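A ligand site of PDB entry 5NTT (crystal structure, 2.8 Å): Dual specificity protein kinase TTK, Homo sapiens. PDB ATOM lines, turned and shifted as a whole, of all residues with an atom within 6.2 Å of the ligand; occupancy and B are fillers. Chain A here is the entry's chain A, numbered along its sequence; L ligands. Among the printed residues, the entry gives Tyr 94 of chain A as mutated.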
ATOM      1  N   LYS A  19      34.339  -6.264 -27.345  1.00  0.00           N
ATOM      2  CA  LYS A  19      34.728  -6.070 -25.952  1.00  0.00           C
ATOM      3  C   LYS A  19      33.557  -6.220 -25.003  1.00  0.00           C
ATOM      4  O   LYS A  19      32.407  -6.248 -25.430  1.00  0.00           O
ATOM      5  CB  LYS A  19      35.378  -4.680 -25.734  1.00  0.00           C
ATOM      6  CG  LYS A  19      34.455  -3.487 -25.862  1.00  0.00           C
ATOM      7  CD  LYS A  19      35.218  -2.200 -25.572  1.00  0.00           C
ATOM      8  CE  LYS A  19      34.384  -0.962 -25.826  1.00  0.00           C
ATOM      9  NZ  LYS A  19      35.216   0.192 -26.301  1.00  0.00           N
ATOM     10  N   GLN A  20      33.876  -6.313 -23.716  1.00  0.00           N
ATOM     11  CA  GLN A  20      32.895  -6.329 -22.645  1.00  0.00           C
ATOM     12  C   GLN A  20      32.696  -4.923 -22.117  1.00  0.00           C
ATOM     13  O   GLN A  20      33.668  -4.269 -21.763  1.00  0.00           O
ATOM     14  CB  GLN A  20      33.389  -7.246 -21.527  1.00  0.00           C
ATOM     15  CG  GLN A  20      32.482  -7.305 -20.304  1.00  0.00           C
ATOM     16  CD  GLN A  20      32.976  -8.308 -19.267  1.00  0.00           C
ATOM     17  OE1 GLN A  20      33.672  -9.286 -19.579  1.00  0.00           O
ATOM     18  NE2 GLN A  20      32.611  -8.067 -18.012  1.00  0.00           N
ATOM     19  N   ILE A  21      31.449  -4.467 -22.040  1.00  0.00           N
ATOM     20  CA  ILE A  21      31.132  -3.067 -21.732  1.00  0.00           C
ATOM     21  C   ILE A  21      30.268  -2.930 -20.485  1.00  0.00           C
ATOM     22  O   ILE A  21      29.503  -1.966 -20.365  1.00  0.00           O
ATOM     23  CB  ILE A  21      30.481  -2.351 -22.965  1.00  0.00           C
ATOM     24  CG1 ILE A  21      29.105  -2.926 -23.316  1.00  0.00           C
ATOM     25  CG2 ILE A  21      31.415  -2.457 -24.159  1.00  0.00           C
ATOM     26  CD1 ILE A  21      28.497  -2.319 -24.563  1.00  0.00           C
ATOM     27  N   GLY A  22      30.410  -3.855 -19.555  1.00  0.00           N
ATOM     28  CA  GLY A  22      29.522  -3.911 -18.388  1.00  0.00           C
ATOM     29  C   GLY A  22      29.392  -5.299 -17.796  1.00  0.00           C
ATOM     30  O   GLY A  22      29.619  -6.308 -18.484  1.00  0.00           O
ATOM     31  N   SER A  23      29.030  -5.330 -16.512  1.00  0.00           N
ATOM     32  CA  SER A  23      28.885  -6.581 -15.763  1.00  0.00           C
ATOM     33  C   SER A  23      28.101  -6.399 -14.450  1.00  0.00           C
ATOM     34  O   SER A  23      28.407  -5.511 -13.657  1.00  0.00           O
ATOM     35  CB  SER A  23      30.265  -7.184 -15.449  1.00  0.00           C
ATOM     36  OG  SER A  23      31.039  -6.293 -14.672  1.00  0.00           O
ATOM     37  N   GLY A  24      27.082  -7.232 -14.254  1.00  0.00           N
ATOM     38  CA  GLY A  24      26.484  -7.483 -12.947  1.00  0.00           C
ATOM     39  C   GLY A  24      27.153  -8.715 -12.330  1.00  0.00           C
ATOM     40  O   GLY A  24      28.245  -9.115 -12.763  1.00  0.00           O
ATOM     41  N   SER A  27      25.648 -11.459 -14.729  1.00  0.00           N
ATOM     42  CA  SER A  27      25.458 -10.935 -16.084  1.00  0.00           C
ATOM     43  C   SER A  27      26.664 -10.177 -16.651  1.00  0.00           C
ATOM     44  O   SER A  27      27.508  -9.661 -15.908  1.00  0.00           O
ATOM     45  CB  SER A  27      24.215 -10.046 -16.119  1.00  0.00           C
ATOM     46  OG  SER A  27      24.315  -9.001 -15.178  1.00  0.00           O
ATOM     47  N   LYS A  28      26.731 -10.130 -17.975  1.00  0.00           N
ATOM     48  CA  LYS A  28      27.760  -9.399 -18.707  1.00  0.00           C
ATOM     49  C   LYS A  28      27.122  -8.693 -19.894  1.00  0.00           C
ATOM     50  O   LYS A  28      26.121  -9.155 -20.417  1.00  0.00           O
ATOM     51  CB  LYS A  28      28.833 -10.355 -19.192  1.00  0.00           C
ATOM     52  CG  LYS A  28      29.616 -11.030 -18.081  1.00  0.00           C
ATOM     53  CD  LYS A  28      30.878 -11.697 -18.613  1.00  0.00           C
ATOM     54  CE  LYS A  28      31.790 -12.239 -17.516  1.00  0.00           C
ATOM     55  NZ  LYS A  28      31.687 -13.710 -17.361  1.00  0.00           N
ATOM     56  N   VAL A  29      27.689  -7.564 -20.327  1.00  0.00           N
ATOM     57  CA  VAL A  29      27.262  -6.919 -21.589  1.00  0.00           C
ATOM     58  C   VAL A  29      28.449  -6.858 -22.538  1.00  0.00           C
ATOM     59  O   VAL A  29      29.558  -6.552 -22.123  1.00  0.00           O
ATOM     60  CB  VAL A  29      26.696  -5.502 -21.361  1.00  0.00           C
ATOM     61  CG1 VAL A  29      26.135  -4.937 -22.661  1.00  0.00           C
ATOM     62  CG2 VAL A  29      25.622  -5.531 -20.276  1.00  0.00           C
ATOM     63  N   GLN A  31      29.927  -5.508 -26.450  1.00  0.00           N
ATOM     64  CA  GLN A  31      29.885  -4.826 -27.749  1.00  0.00           C
ATOM     65  C   GLN A  31      30.200  -5.876 -28.818  1.00  0.00           C
ATOM     66  O   GLN A  31      31.278  -6.485 -28.787  1.00  0.00           O
ATOM     67  CB  GLN A  31      30.908  -3.678 -27.792  1.00  0.00           C
ATOM     68  CG  GLN A  31      30.795  -2.755 -29.000  1.00  0.00           C
ATOM     69  CD  GLN A  31      31.972  -1.789 -29.113  1.00  0.00           C
ATOM     70  OE1 GLN A  31      33.132  -2.198 -29.011  1.00  0.00           O
ATOM     71  NE2 GLN A  31      31.681  -0.501 -29.353  1.00  0.00           N
ATOM     72  N   TYR A  40      25.803  -4.256 -32.116  1.00  0.00           N
ATOM     73  CA  TYR A  40      24.816  -4.472 -31.072  1.00  0.00           C
ATOM     74  C   TYR A  40      25.516  -4.584 -29.720  1.00  0.00           C
ATOM     75  O   TYR A  40      26.759  -4.684 -29.637  1.00  0.00           O
ATOM     76  CB  TYR A  40      24.031  -5.777 -31.324  1.00  0.00           C
ATOM     77  CG  TYR A  40      23.359  -5.857 -32.679  1.00  0.00           C
ATOM     78  CD1 TYR A  40      22.084  -5.329 -32.869  1.00  0.00           C
ATOM     79  CD2 TYR A  40      23.997  -6.446 -33.771  1.00  0.00           C
ATOM     80  CE1 TYR A  40      21.470  -5.379 -34.106  1.00  0.00           C
ATOM     81  CE2 TYR A  40      23.378  -6.508 -35.014  1.00  0.00           C
ATOM     82  CZ  TYR A  40      22.113  -5.973 -35.175  1.00  0.00           C
ATOM     83  OH  TYR A  40      21.489  -6.014 -36.408  1.00  0.00           O
ATOM     84  N   ALA A  41      24.699  -4.538 -28.684  1.00  0.00           N
ATOM     85  CA  ALA A  41      25.112  -4.945 -27.339  1.00  0.00           C
ATOM     86  C   ALA A  41      24.399  -6.244 -27.038  1.00  0.00           C
ATOM     87  O   ALA A  41      23.190  -6.350 -27.272  1.00  0.00           O
ATOM     88  CB  ALA A  41      24.756  -3.879 -26.320  1.00  0.00           C
ATOM     89  N   LYS A  43      23.448  -8.631 -23.907  1.00  0.00           N
ATOM     90  CA  LYS A  43      23.405  -8.934 -22.482  1.00  0.00           C
ATOM     91  C   LYS A  43      23.395 -10.441 -22.326  1.00  0.00           C
ATOM     92  O   LYS A  43      22.585 -11.123 -22.938  1.00  0.00           O
ATOM     93  CB  LYS A  43      22.148  -8.342 -21.852  1.00  0.00           C
ATOM     94  CG  LYS A  43      22.148  -8.283 -20.336  1.00  0.00           C
ATOM     95  CD  LYS A  43      20.774  -7.882 -19.803  1.00  0.00           C
ATOM     96  CE  LYS A  43      20.836  -6.855 -18.691  1.00  0.00           C
ATOM     97  NZ  LYS A  43      19.637  -5.967 -18.656  1.00  0.00           N
ATOM     98  N   TYR A  44      24.319 -10.962 -21.527  1.00  0.00           N
ATOM     99  CA  TYR A  44      24.331 -12.373 -21.139  1.00  0.00           C
ATOM    100  C   TYR A  44      23.948 -12.446 -19.664  1.00  0.00           C
ATOM    101  O   TYR A  44      24.441 -11.640 -18.867  1.00  0.00           O
ATOM    102  CB  TYR A  44      25.724 -12.973 -21.357  1.00  0.00           C
ATOM    103  CG  TYR A  44      26.025 -14.211 -20.540  1.00  0.00           C
ATOM    104  CD1 TYR A  44      25.524 -15.447 -20.903  1.00  0.00           C
ATOM    105  CD2 TYR A  44      26.845 -14.136 -19.414  1.00  0.00           C
ATOM    106  CE1 TYR A  44      25.814 -16.586 -20.161  1.00  0.00           C
ATOM    107  CE2 TYR A  44      27.148 -15.273 -18.671  1.00  0.00           C
ATOM    108  CZ  TYR A  44      26.632 -16.494 -19.052  1.00  0.00           C
ATOM    109  OH  TYR A  44      26.915 -17.628 -18.333  1.00  0.00           O
ATOM    110  N   ILE A  76      14.745   0.923 -25.238  1.00  0.00           N
ATOM    111  CA  ILE A  76      15.835   0.264 -25.976  1.00  0.00           C
ATOM    112  C   ILE A  76      15.300  -0.881 -26.846  1.00  0.00           C
ATOM    113  O   ILE A  76      14.383  -1.577 -26.432  1.00  0.00           O
ATOM    114  CB  ILE A  76      16.915  -0.242 -25.004  1.00  0.00           C
ATOM    115  CG1 ILE A  76      18.215  -0.531 -25.764  1.00  0.00           C
ATOM    116  CG2 ILE A  76      16.443  -1.456 -24.209  1.00  0.00           C
ATOM    117  CD1 ILE A  76      19.380  -0.805 -24.841  1.00  0.00           C
ATOM    118  N   MET A  92      20.622  -6.455 -28.277  1.00  0.00           N
ATOM    119  CA  MET A  92      20.025  -5.162 -28.025  1.00  0.00           C
ATOM    120  C   MET A  92      20.718  -4.035 -28.762  1.00  0.00           C
ATOM    121  O   MET A  92      21.869  -4.165 -29.181  1.00  0.00           O
ATOM    122  CB  MET A  92      20.046  -4.887 -26.526  1.00  0.00           C
ATOM    123  CG  MET A  92      19.388  -5.996 -25.717  1.00  0.00           C
ATOM    124  SD  MET A  92      19.001  -5.490 -24.045  1.00  0.00           S
ATOM    125  CE  MET A  92      20.662  -5.247 -23.453  1.00  0.00           C
ATOM    126  N   GLU A  93      19.983  -2.933 -28.884  1.00  0.00           N
ATOM    127  CA  GLU A  93      20.481  -1.676 -29.460  1.00  0.00           C
ATOM    128  C   GLU A  93      21.754  -1.209 -28.750  1.00  0.00           C
ATOM    129  O   GLU A  93      21.846  -1.290 -27.533  1.00  0.00           O
ATOM    130  CB  GLU A  93      19.378  -0.634 -29.338  1.00  0.00           C
ATOM    131  CG  GLU A  93      19.639   0.765 -29.882  1.00  0.00           C
ATOM    132  CD  GLU A  93      18.357   1.582 -29.996  1.00  0.00           C
ATOM    133  OE1 GLU A  93      17.396   1.367 -29.200  1.00  0.00           O
ATOM    134  OE2 GLU A  93      18.293   2.454 -30.895  1.00  0.00           O
ATOM    135  N   TYR A  94      22.738  -0.771 -29.527  1.00  0.00           N
ATOM    136  CA  TYR A  94      23.994  -0.255 -28.993  1.00  0.00           C
ATOM    137  C   TYR A  94      23.911   1.257 -28.793  1.00  0.00           C
ATOM    138  O   TYR A  94      23.324   1.962 -29.621  1.00  0.00           O
ATOM    139  CB  TYR A  94      25.147  -0.609 -29.930  1.00  0.00           C
ATOM    140  CG  TYR A  94      26.450   0.034 -29.540  1.00  0.00           C
ATOM    141  CD1 TYR A  94      27.259  -0.535 -28.551  1.00  0.00           C
ATOM    142  CD2 TYR A  94      26.869   1.213 -30.134  1.00  0.00           C
ATOM    143  CE1 TYR A  94      28.449   0.057 -28.172  1.00  0.00           C
ATOM    144  CE2 TYR A  94      28.066   1.814 -29.762  1.00  0.00           C
ATOM    145  CZ  TYR A  94      28.850   1.229 -28.788  1.00  0.00           C
ATOM    146  OH  TYR A  94      30.034   1.818 -28.417  1.00  0.00           O
ATOM    147  N   GLY A  95      24.502   1.741 -27.697  1.00  0.00           N
ATOM    148  CA  GLY A  95      24.738   3.179 -27.459  1.00  0.00           C
ATOM    149  C   GLY A  95      26.182   3.427 -27.049  1.00  0.00           C
ATOM    150  O   GLY A  95      26.787   2.580 -26.406  1.00  0.00           O
ATOM    151  N   ASN A  96      26.739   4.578 -27.401  1.00  0.00           N
ATOM    152  CA  ASN A  96      28.157   4.847 -27.084  1.00  0.00           C
ATOM    153  C   ASN A  96      28.372   5.221 -25.615  1.00  0.00           C
ATOM    154  O   ASN A  96      29.497   5.114 -25.112  1.00  0.00           O
ATOM    155  CB  ASN A  96      28.764   5.902 -28.034  1.00  0.00           C
ATOM    156  CG  ASN A  96      30.270   5.712 -28.247  1.00  0.00           C
ATOM    157  OD1 ASN A  96      30.734   4.601 -28.513  1.00  0.00           O
ATOM    158  ND2 ASN A  96      31.040   6.803 -28.142  1.00  0.00           N
ATOM    159  N   ILE A  97      27.318   5.660 -24.933  1.00  0.00           N
ATOM    160  CA  ILE A  97      27.416   6.073 -23.541  1.00  0.00           C
ATOM    161  C   ILE A  97      26.047   6.101 -22.856  1.00  0.00           C
ATOM    162  O   ILE A  97      25.014   6.320 -23.511  1.00  0.00           O
ATOM    163  CB  ILE A  97      28.112   7.460 -23.440  1.00  0.00           C
ATOM    164  CG1 ILE A  97      28.782   7.624 -22.070  1.00  0.00           C
ATOM    165  CG2 ILE A  97      27.138   8.598 -23.722  1.00  0.00           C
ATOM    166  CD1 ILE A  97      29.596   8.895 -21.924  1.00  0.00           C
ATOM    167  N   ASP A  98      26.044   5.857 -21.537  1.00  0.00           N
ATOM    168  CA  ASP A  98      24.837   6.007 -20.717  1.00  0.00           C
ATOM    169  C   ASP A  98      24.791   7.403 -20.099  1.00  0.00           C
ATOM    170  O   ASP A  98      25.800   8.119 -20.075  1.00  0.00           O
ATOM    171  CB  ASP A  98      24.703   4.883 -19.669  1.00  0.00           C
ATOM    172  CG  ASP A  98      25.701   5.001 -18.517  1.00  0.00           C
ATOM    173  OD1 ASP A  98      26.704   5.724 -18.624  1.00  0.00           O
ATOM    174  OD2 ASP A  98      25.480   4.332 -17.485  1.00  0.00           O
ATOM    175  N   SER A 101      27.362   8.303 -17.074  1.00  0.00           N
ATOM    176  CA  SER A 101      28.728   8.613 -17.473  1.00  0.00           C
ATOM    177  C   SER A 101      28.808   9.938 -18.206  1.00  0.00           C
ATOM    178  O   SER A 101      29.741  10.708 -17.975  1.00  0.00           O
ATOM    179  CB  SER A 101      29.289   7.513 -18.357  1.00  0.00           C
ATOM    180  OG  SER A 101      29.102   6.266 -17.720  1.00  0.00           O
ATOM    181  N   TRP A 102      27.843  10.203 -19.077  1.00  0.00           N
ATOM    182  CA  TRP A 102      27.770  11.486 -19.790  1.00  0.00           C
ATOM    183  C   TRP A 102      27.675  12.687 -18.829  1.00  0.00           C
ATOM    184  O   TRP A 102      28.368  13.693 -19.022  1.00  0.00           O
ATOM    185  CB  TRP A 102      26.592  11.492 -20.765  1.00  0.00           C
ATOM    186  CG  TRP A 102      26.463  12.782 -21.500  1.00  0.00           C
ATOM    187  CD1 TRP A 102      25.466  13.701 -21.361  1.00  0.00           C
ATOM    188  CD2 TRP A 102      27.373  13.310 -22.457  1.00  0.00           C
ATOM    189  NE1 TRP A 102      25.706  14.779 -22.189  1.00  0.00           N
ATOM    190  CE2 TRP A 102      26.867  14.552 -22.879  1.00  0.00           C
ATOM    191  CE3 TRP A 102      28.573  12.845 -23.012  1.00  0.00           C
ATOM    192  CZ2 TRP A 102      27.520  15.347 -23.827  1.00  0.00           C
ATOM    193  CZ3 TRP A 102      29.227  13.631 -23.959  1.00  0.00           C
ATOM    194  CH2 TRP A 102      28.691  14.872 -24.354  1.00  0.00           C
ATOM    195  N   LYS A 105      31.030  13.561 -16.926  1.00  0.00           N
ATOM    196  CA  LYS A 105      31.949  14.342 -17.742  1.00  0.00           C
ATOM    197  C   LYS A 105      31.366  15.618 -18.365  1.00  0.00           C
ATOM    198  O   LYS A 105      31.906  16.132 -19.345  1.00  0.00           O
ATOM    199  CB  LYS A 105      32.561  13.449 -18.840  1.00  0.00           C
ATOM    200  CG  LYS A 105      31.624  13.017 -19.958  1.00  0.00           C
ATOM    201  CD  LYS A 105      32.417  12.432 -21.114  1.00  0.00           C
ATOM    202  CE  LYS A 105      33.061  11.088 -20.762  1.00  0.00           C
ATOM    203  NZ  LYS A 105      34.520  11.013 -21.092  1.00  0.00           N
ATOM    204  N   LYS A 139      17.608   5.692 -12.044  1.00  0.00           N
ATOM    205  CA  LYS A 139      18.828   6.462 -11.906  1.00  0.00           C
ATOM    206  C   LYS A 139      19.258   6.819 -13.334  1.00  0.00           C
ATOM    207  O   LYS A 139      18.754   6.228 -14.295  1.00  0.00           O
ATOM    208  CB  LYS A 139      19.916   5.639 -11.229  1.00  0.00           C
ATOM    209  CG  LYS A 139      19.489   4.861  -9.979  1.00  0.00           C
ATOM    210  CD  LYS A 139      20.356   3.633  -9.701  1.00  0.00           C
ATOM    211  CE  LYS A 139      20.283   2.530 -10.767  1.00  0.00           C
ATOM    212  NZ  LYS A 139      18.953   1.869 -10.941  1.00  0.00           N
ATOM    213  N   ALA A 141      21.879   5.868 -14.834  1.00  0.00           N
ATOM    214  CA  ALA A 141      22.420   4.631 -15.418  1.00  0.00           C
ATOM    215  C   ALA A 141      21.385   3.760 -16.132  1.00  0.00           C
ATOM    216  O   ALA A 141      21.762   2.944 -16.979  1.00  0.00           O
ATOM    217  CB  ALA A 141      23.133   3.802 -14.362  1.00  0.00           C
ATOM    218  N   ASN A 142      20.111   3.927 -15.797  1.00  0.00           N
ATOM    219  CA  ASN A 142      19.032   3.216 -16.499  1.00  0.00           C
ATOM    220  C   ASN A 142      18.707   3.786 -17.875  1.00  0.00           C
ATOM    221  O   ASN A 142      17.873   3.238 -18.576  1.00  0.00           O
ATOM    222  CB  ASN A 142      17.767   3.180 -15.627  1.00  0.00           C
ATOM    223  CG  ASN A 142      17.967   2.421 -14.328  1.00  0.00           C
ATOM    224  OD1 ASN A 142      18.065   3.015 -13.259  1.00  0.00           O
ATOM    225  ND2 ASN A 142      18.064   1.106 -14.414  1.00  0.00           N
ATOM    226  N   LEU A 144      20.233   5.085 -21.652  1.00  0.00           N
ATOM    227  CA  LEU A 144      21.303   4.928 -22.622  1.00  0.00           C
ATOM    228  C   LEU A 144      21.157   6.005 -23.677  1.00  0.00           C
ATOM    229  O   LEU A 144      20.064   6.220 -24.187  1.00  0.00           O
ATOM    230  CB  LEU A 144      21.166   3.566 -23.286  1.00  0.00           C
ATOM    231  CG  LEU A 144      22.292   3.107 -24.210  1.00  0.00           C
ATOM    232  CD1 LEU A 144      23.539   2.786 -23.394  1.00  0.00           C
ATOM    233  CD2 LEU A 144      21.851   1.903 -25.032  1.00  0.00           C
ATOM    234  N   ILE A 153      16.663   1.409 -20.490  1.00  0.00           N
ATOM    235  CA  ILE A 153      17.351   0.120 -20.632  1.00  0.00           C
ATOM    236  C   ILE A 153      16.575  -1.026 -19.980  1.00  0.00           C
ATOM    237  O   ILE A 153      16.496  -2.113 -20.538  1.00  0.00           O
ATOM    238  CB  ILE A 153      18.760   0.191 -20.018  1.00  0.00           C
ATOM    239  CG1 ILE A 153      19.648   1.141 -20.836  1.00  0.00           C
ATOM    240  CG2 ILE A 153      19.425  -1.179 -19.956  1.00  0.00           C
ATOM    241  CD1 ILE A 153      20.889   1.618 -20.102  1.00  0.00           C
ATOM    242  N   ASP A 154      16.034  -0.782 -18.781  1.00  0.00           N
ATOM    243  CA  ASP A 154      15.306  -1.798 -18.022  1.00  0.00           C
ATOM    244  C   ASP A 154      14.034  -1.214 -17.364  1.00  0.00           C
ATOM    245  O   ASP A 154      13.842   0.004 -17.331  1.00  0.00           O
ATOM    246  CB  ASP A 154      16.235  -2.418 -16.970  1.00  0.00           C
ATOM    247  CG  ASP A 154      16.527  -1.498 -15.802  1.00  0.00           C
ATOM    248  OD1 ASP A 154      16.622  -0.278 -16.034  1.00  0.00           O
ATOM    249  OD2 ASP A 154      16.660  -1.985 -14.653  1.00  0.00           O
ATOM    250  N   GLN A 160      17.605  -8.545  -8.644  1.00  0.00           N
ATOM    251  CA  GLN A 160      19.061  -8.432  -8.722  1.00  0.00           C
ATOM    252  C   GLN A 160      19.725  -9.605  -8.000  1.00  0.00           C
ATOM    253  O   GLN A 160      19.116 -10.218  -7.105  1.00  0.00           O
ATOM    254  CB  GLN A 160      19.533  -7.098  -8.126  1.00  0.00           C
ATOM    255  CG  GLN A 160      18.939  -5.836  -8.761  1.00  0.00           C
ATOM    256  CD  GLN A 160      19.399  -5.601 -10.203  1.00  0.00           C
ATOM    257  OE1 GLN A 160      20.541  -5.907 -10.559  1.00  0.00           O
ATOM    258  NE2 GLN A 160      18.514  -5.045 -11.018  1.00  0.00           N
HETATM  259  C1  LIG L   1      22.158  -2.405 -22.078  1.00  0.00           C
HETATM  260  C2  LIG L   1      22.601  -2.194 -23.525  1.00  0.00           C
HETATM  261  C3  LIG L   1      23.246  -2.155 -21.080  1.00  0.00           C
HETATM  262  C4  LIG L   1      24.387  -1.459 -21.414  1.00  0.00           C
HETATM  263  N1  LIG L   1      25.152  -1.402 -20.276  1.00  0.00           N
HETATM  264  N2  LIG L   1      24.533  -2.022 -19.237  1.00  0.00           N
HETATM  265  C5  LIG L   1      23.369  -2.466 -19.737  1.00  0.00           C
HETATM  266  C6  LIG L   1      22.421  -3.223 -18.877  1.00  0.00           C
HETATM  267  N3  LIG L   1      22.817  -3.386 -17.593  1.00  0.00           N
HETATM  268  O1  LIG L   1      21.377  -3.671 -19.342  1.00  0.00           O
HETATM  269  C7  LIG L   1      26.466  -0.795 -20.044  1.00  0.00           C
HETATM  270  C8  LIG L   1      24.670  -0.990 -22.702  1.00  0.00           C
HETATM  271  C9  LIG L   1      23.808  -1.347 -23.760  1.00  0.00           C
HETATM  272  C10 LIG L   1      24.129  -0.889 -25.035  1.00  0.00           C
HETATM  273  N4  LIG L   1      25.218  -0.152 -25.258  1.00  0.00           N
HETATM  274  C11 LIG L   1      26.000   0.130 -24.205  1.00  0.00           C
HETATM  275  N5  LIG L   1      25.772  -0.274 -22.942  1.00  0.00           N
HETATM  276  N6  LIG L   1      27.119   0.880 -24.376  1.00  0.00           N
HETATM  277  C12 LIG L   1      27.830   1.646 -23.428  1.00  0.00           C
HETATM  278  C13 LIG L   1      29.201   1.880 -23.621  1.00  0.00           C
HETATM  279  C14 LIG L   1      29.878   2.639 -22.682  1.00  0.00           C
HETATM  280  C15 LIG L   1      29.229   3.159 -21.559  1.00  0.00           C
HETATM  281  C16 LIG L   1      27.876   2.915 -21.391  1.00  0.00           C
HETATM  282  C17 LIG L   1      27.173   2.175 -22.314  1.00  0.00           C
HETATM  283  O2  LIG L   1      29.738   1.315 -24.771  1.00  0.00           O
HETATM  284  C18 LIG L   1      29.923   3.980 -20.520  1.00  0.00           C
HETATM  285  N7  LIG L   1      31.291   4.122 -20.642  1.00  0.00           N
HETATM  286  O3  LIG L   1      29.270   4.502 -19.621  1.00  0.00           O
HETATM  287  C19 LIG L   1      32.055   5.105 -19.858  1.00  0.00           C
HETATM  288  C20 LIG L   1      33.209   4.448 -19.114  1.00  0.00           C
HETATM  289  C21 LIG L   1      33.992   5.494 -18.339  1.00  0.00           C
HETATM  290  N8  LIG L   1      34.491   6.554 -19.215  1.00  0.00           N
HETATM  291  C22 LIG L   1      33.383   7.223 -19.934  1.00  0.00           C
HETATM  292  C23 LIG L   1      32.582   6.219 -20.747  1.00  0.00           C
HETATM  293  C24 LIG L   1      35.308   7.540 -18.462  1.00  0.00           C
HETATM  294  C25 LIG L   1      31.062   1.284 -24.963  1.00  0.00           C
HETATM  295  F1  LIG L   1      31.742   0.816 -23.925  1.00  0.00           F
HETATM  296  F2  LIG L   1      31.573   2.468 -25.260  1.00  0.00           F
HETATM  297  F3  LIG L   1      31.346   0.505 -25.984  1.00  0.00           F
HETATM  298  C26 LIG L   1      22.081  -4.002 -16.538  1.00  0.00           C
HETATM  299  C27 LIG L   1      22.443  -5.288 -16.118  1.00  0.00           C
HETATM  300  C28 LIG L   1      21.693  -5.858 -15.079  1.00  0.00           C
HETATM  301  C29 LIG L   1      20.648  -5.186 -14.490  1.00  0.00           C
HETATM  302  C30 LIG L   1      20.314  -3.929 -14.924  1.00  0.00           C
HETATM  303  C31 LIG L   1      21.016  -3.294 -15.957  1.00  0.00           C
HETATM  304  C32 LIG L   1      20.599  -1.904 -16.378  1.00  0.00           C
HETATM  305  C33 LIG L   1      21.275  -0.761 -15.650  1.00  0.00           C
HETATM  306  C34 LIG L   1      23.575  -6.065 -16.747  1.00  0.00           C
HETATM  307  C35 LIG L   1      24.959  -5.719 -16.251  1.00  0.00           C
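The side-chain hydroxyl (OH) of Tyr 94 is in hydrogen-bond range of the side-chain amide oxygen (OD1) of Asn 96 (2.9 Å).
The side-chain hydroxyl (OH) of Tyr 94 lies within hydrogen-bond range of the side-chain amide nitrogen (NE2) of Gln 31.
The backbone carbonyl oxygen of Val 29 lies within hydrogen-bond range of the backbone NH of Ile 21 (2.8 Å).
N of Gly 24 sits at hydrogen-bond distance from OG of Ser 27, at 3.4 Å.
The backbone NH of Met 92 sits at hydrogen-bond distance from the backbone carbonyl oxygen of Ala 41 (2.8 Å).
The backbone carbonyl oxygen (O) of Lys 19 lies within hydrogen-bond range of the backbone NH (N) of Gln 31.
N of Val 29 lies within hydrogen-bond range of O of Gly 22 (2.9 Å).
The side-chain amide oxygen of Asn 142 lies within hydrogen-bond range of the side-chain amino group of Lys 139.
The side-chain hydroxyl of Ser 101 lies within hydrogen-bond range of an oxygen (O3) of the ligand.
The backbone NH of Gly 95 is in hydrogen-bond range of a nitrogen (N4) of the ligand (3.2 Å).
The backbone carbonyl oxygen of Gly 95 lies within hydrogen-bond range of a nitrogen (N6) of the ligand (2.7 Å).
NZ of Lys 43 sits at hydrogen-bond distance from O1 of the ligand (3.0 Å).
A fluorine (F3) of the ligand sits close to the side-chain hydroxyl (OH) of Tyr 94 (3.1 Å).
The backbone carbonyl oxygen (O) of Asn 96 sits close to a fluorine (F2) of the ligand (3.4 Å).
An oxygen (O3) of the ligand lies close to the side-chain carboxylate (OD1) of Asp 98 (3.0 Å).
Merely in contact with the ligand: Ile 153, Ile 21, Gly 24, Ala 41, Lys 19, Glu 93, Ser 27, Met 92, Gln 31, Leu 144, Ser 23, Ile 76, Val 29, Ile 97, Asn 142, Lys 105, Ala 141 and Gln 160.
Hydrophobic or aromatic side chains that line the ligand: Ile 21, Val 29, Ala 41, Ile 76, Met 92, Tyr 94, Ile 97, Leu 144 and Ile 153.
Of the 32 residues printed, 24 come within 4 Å of the ligand.
The nearest printed residue that does not touch the ligand is Asp 154 (4.1 Å).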
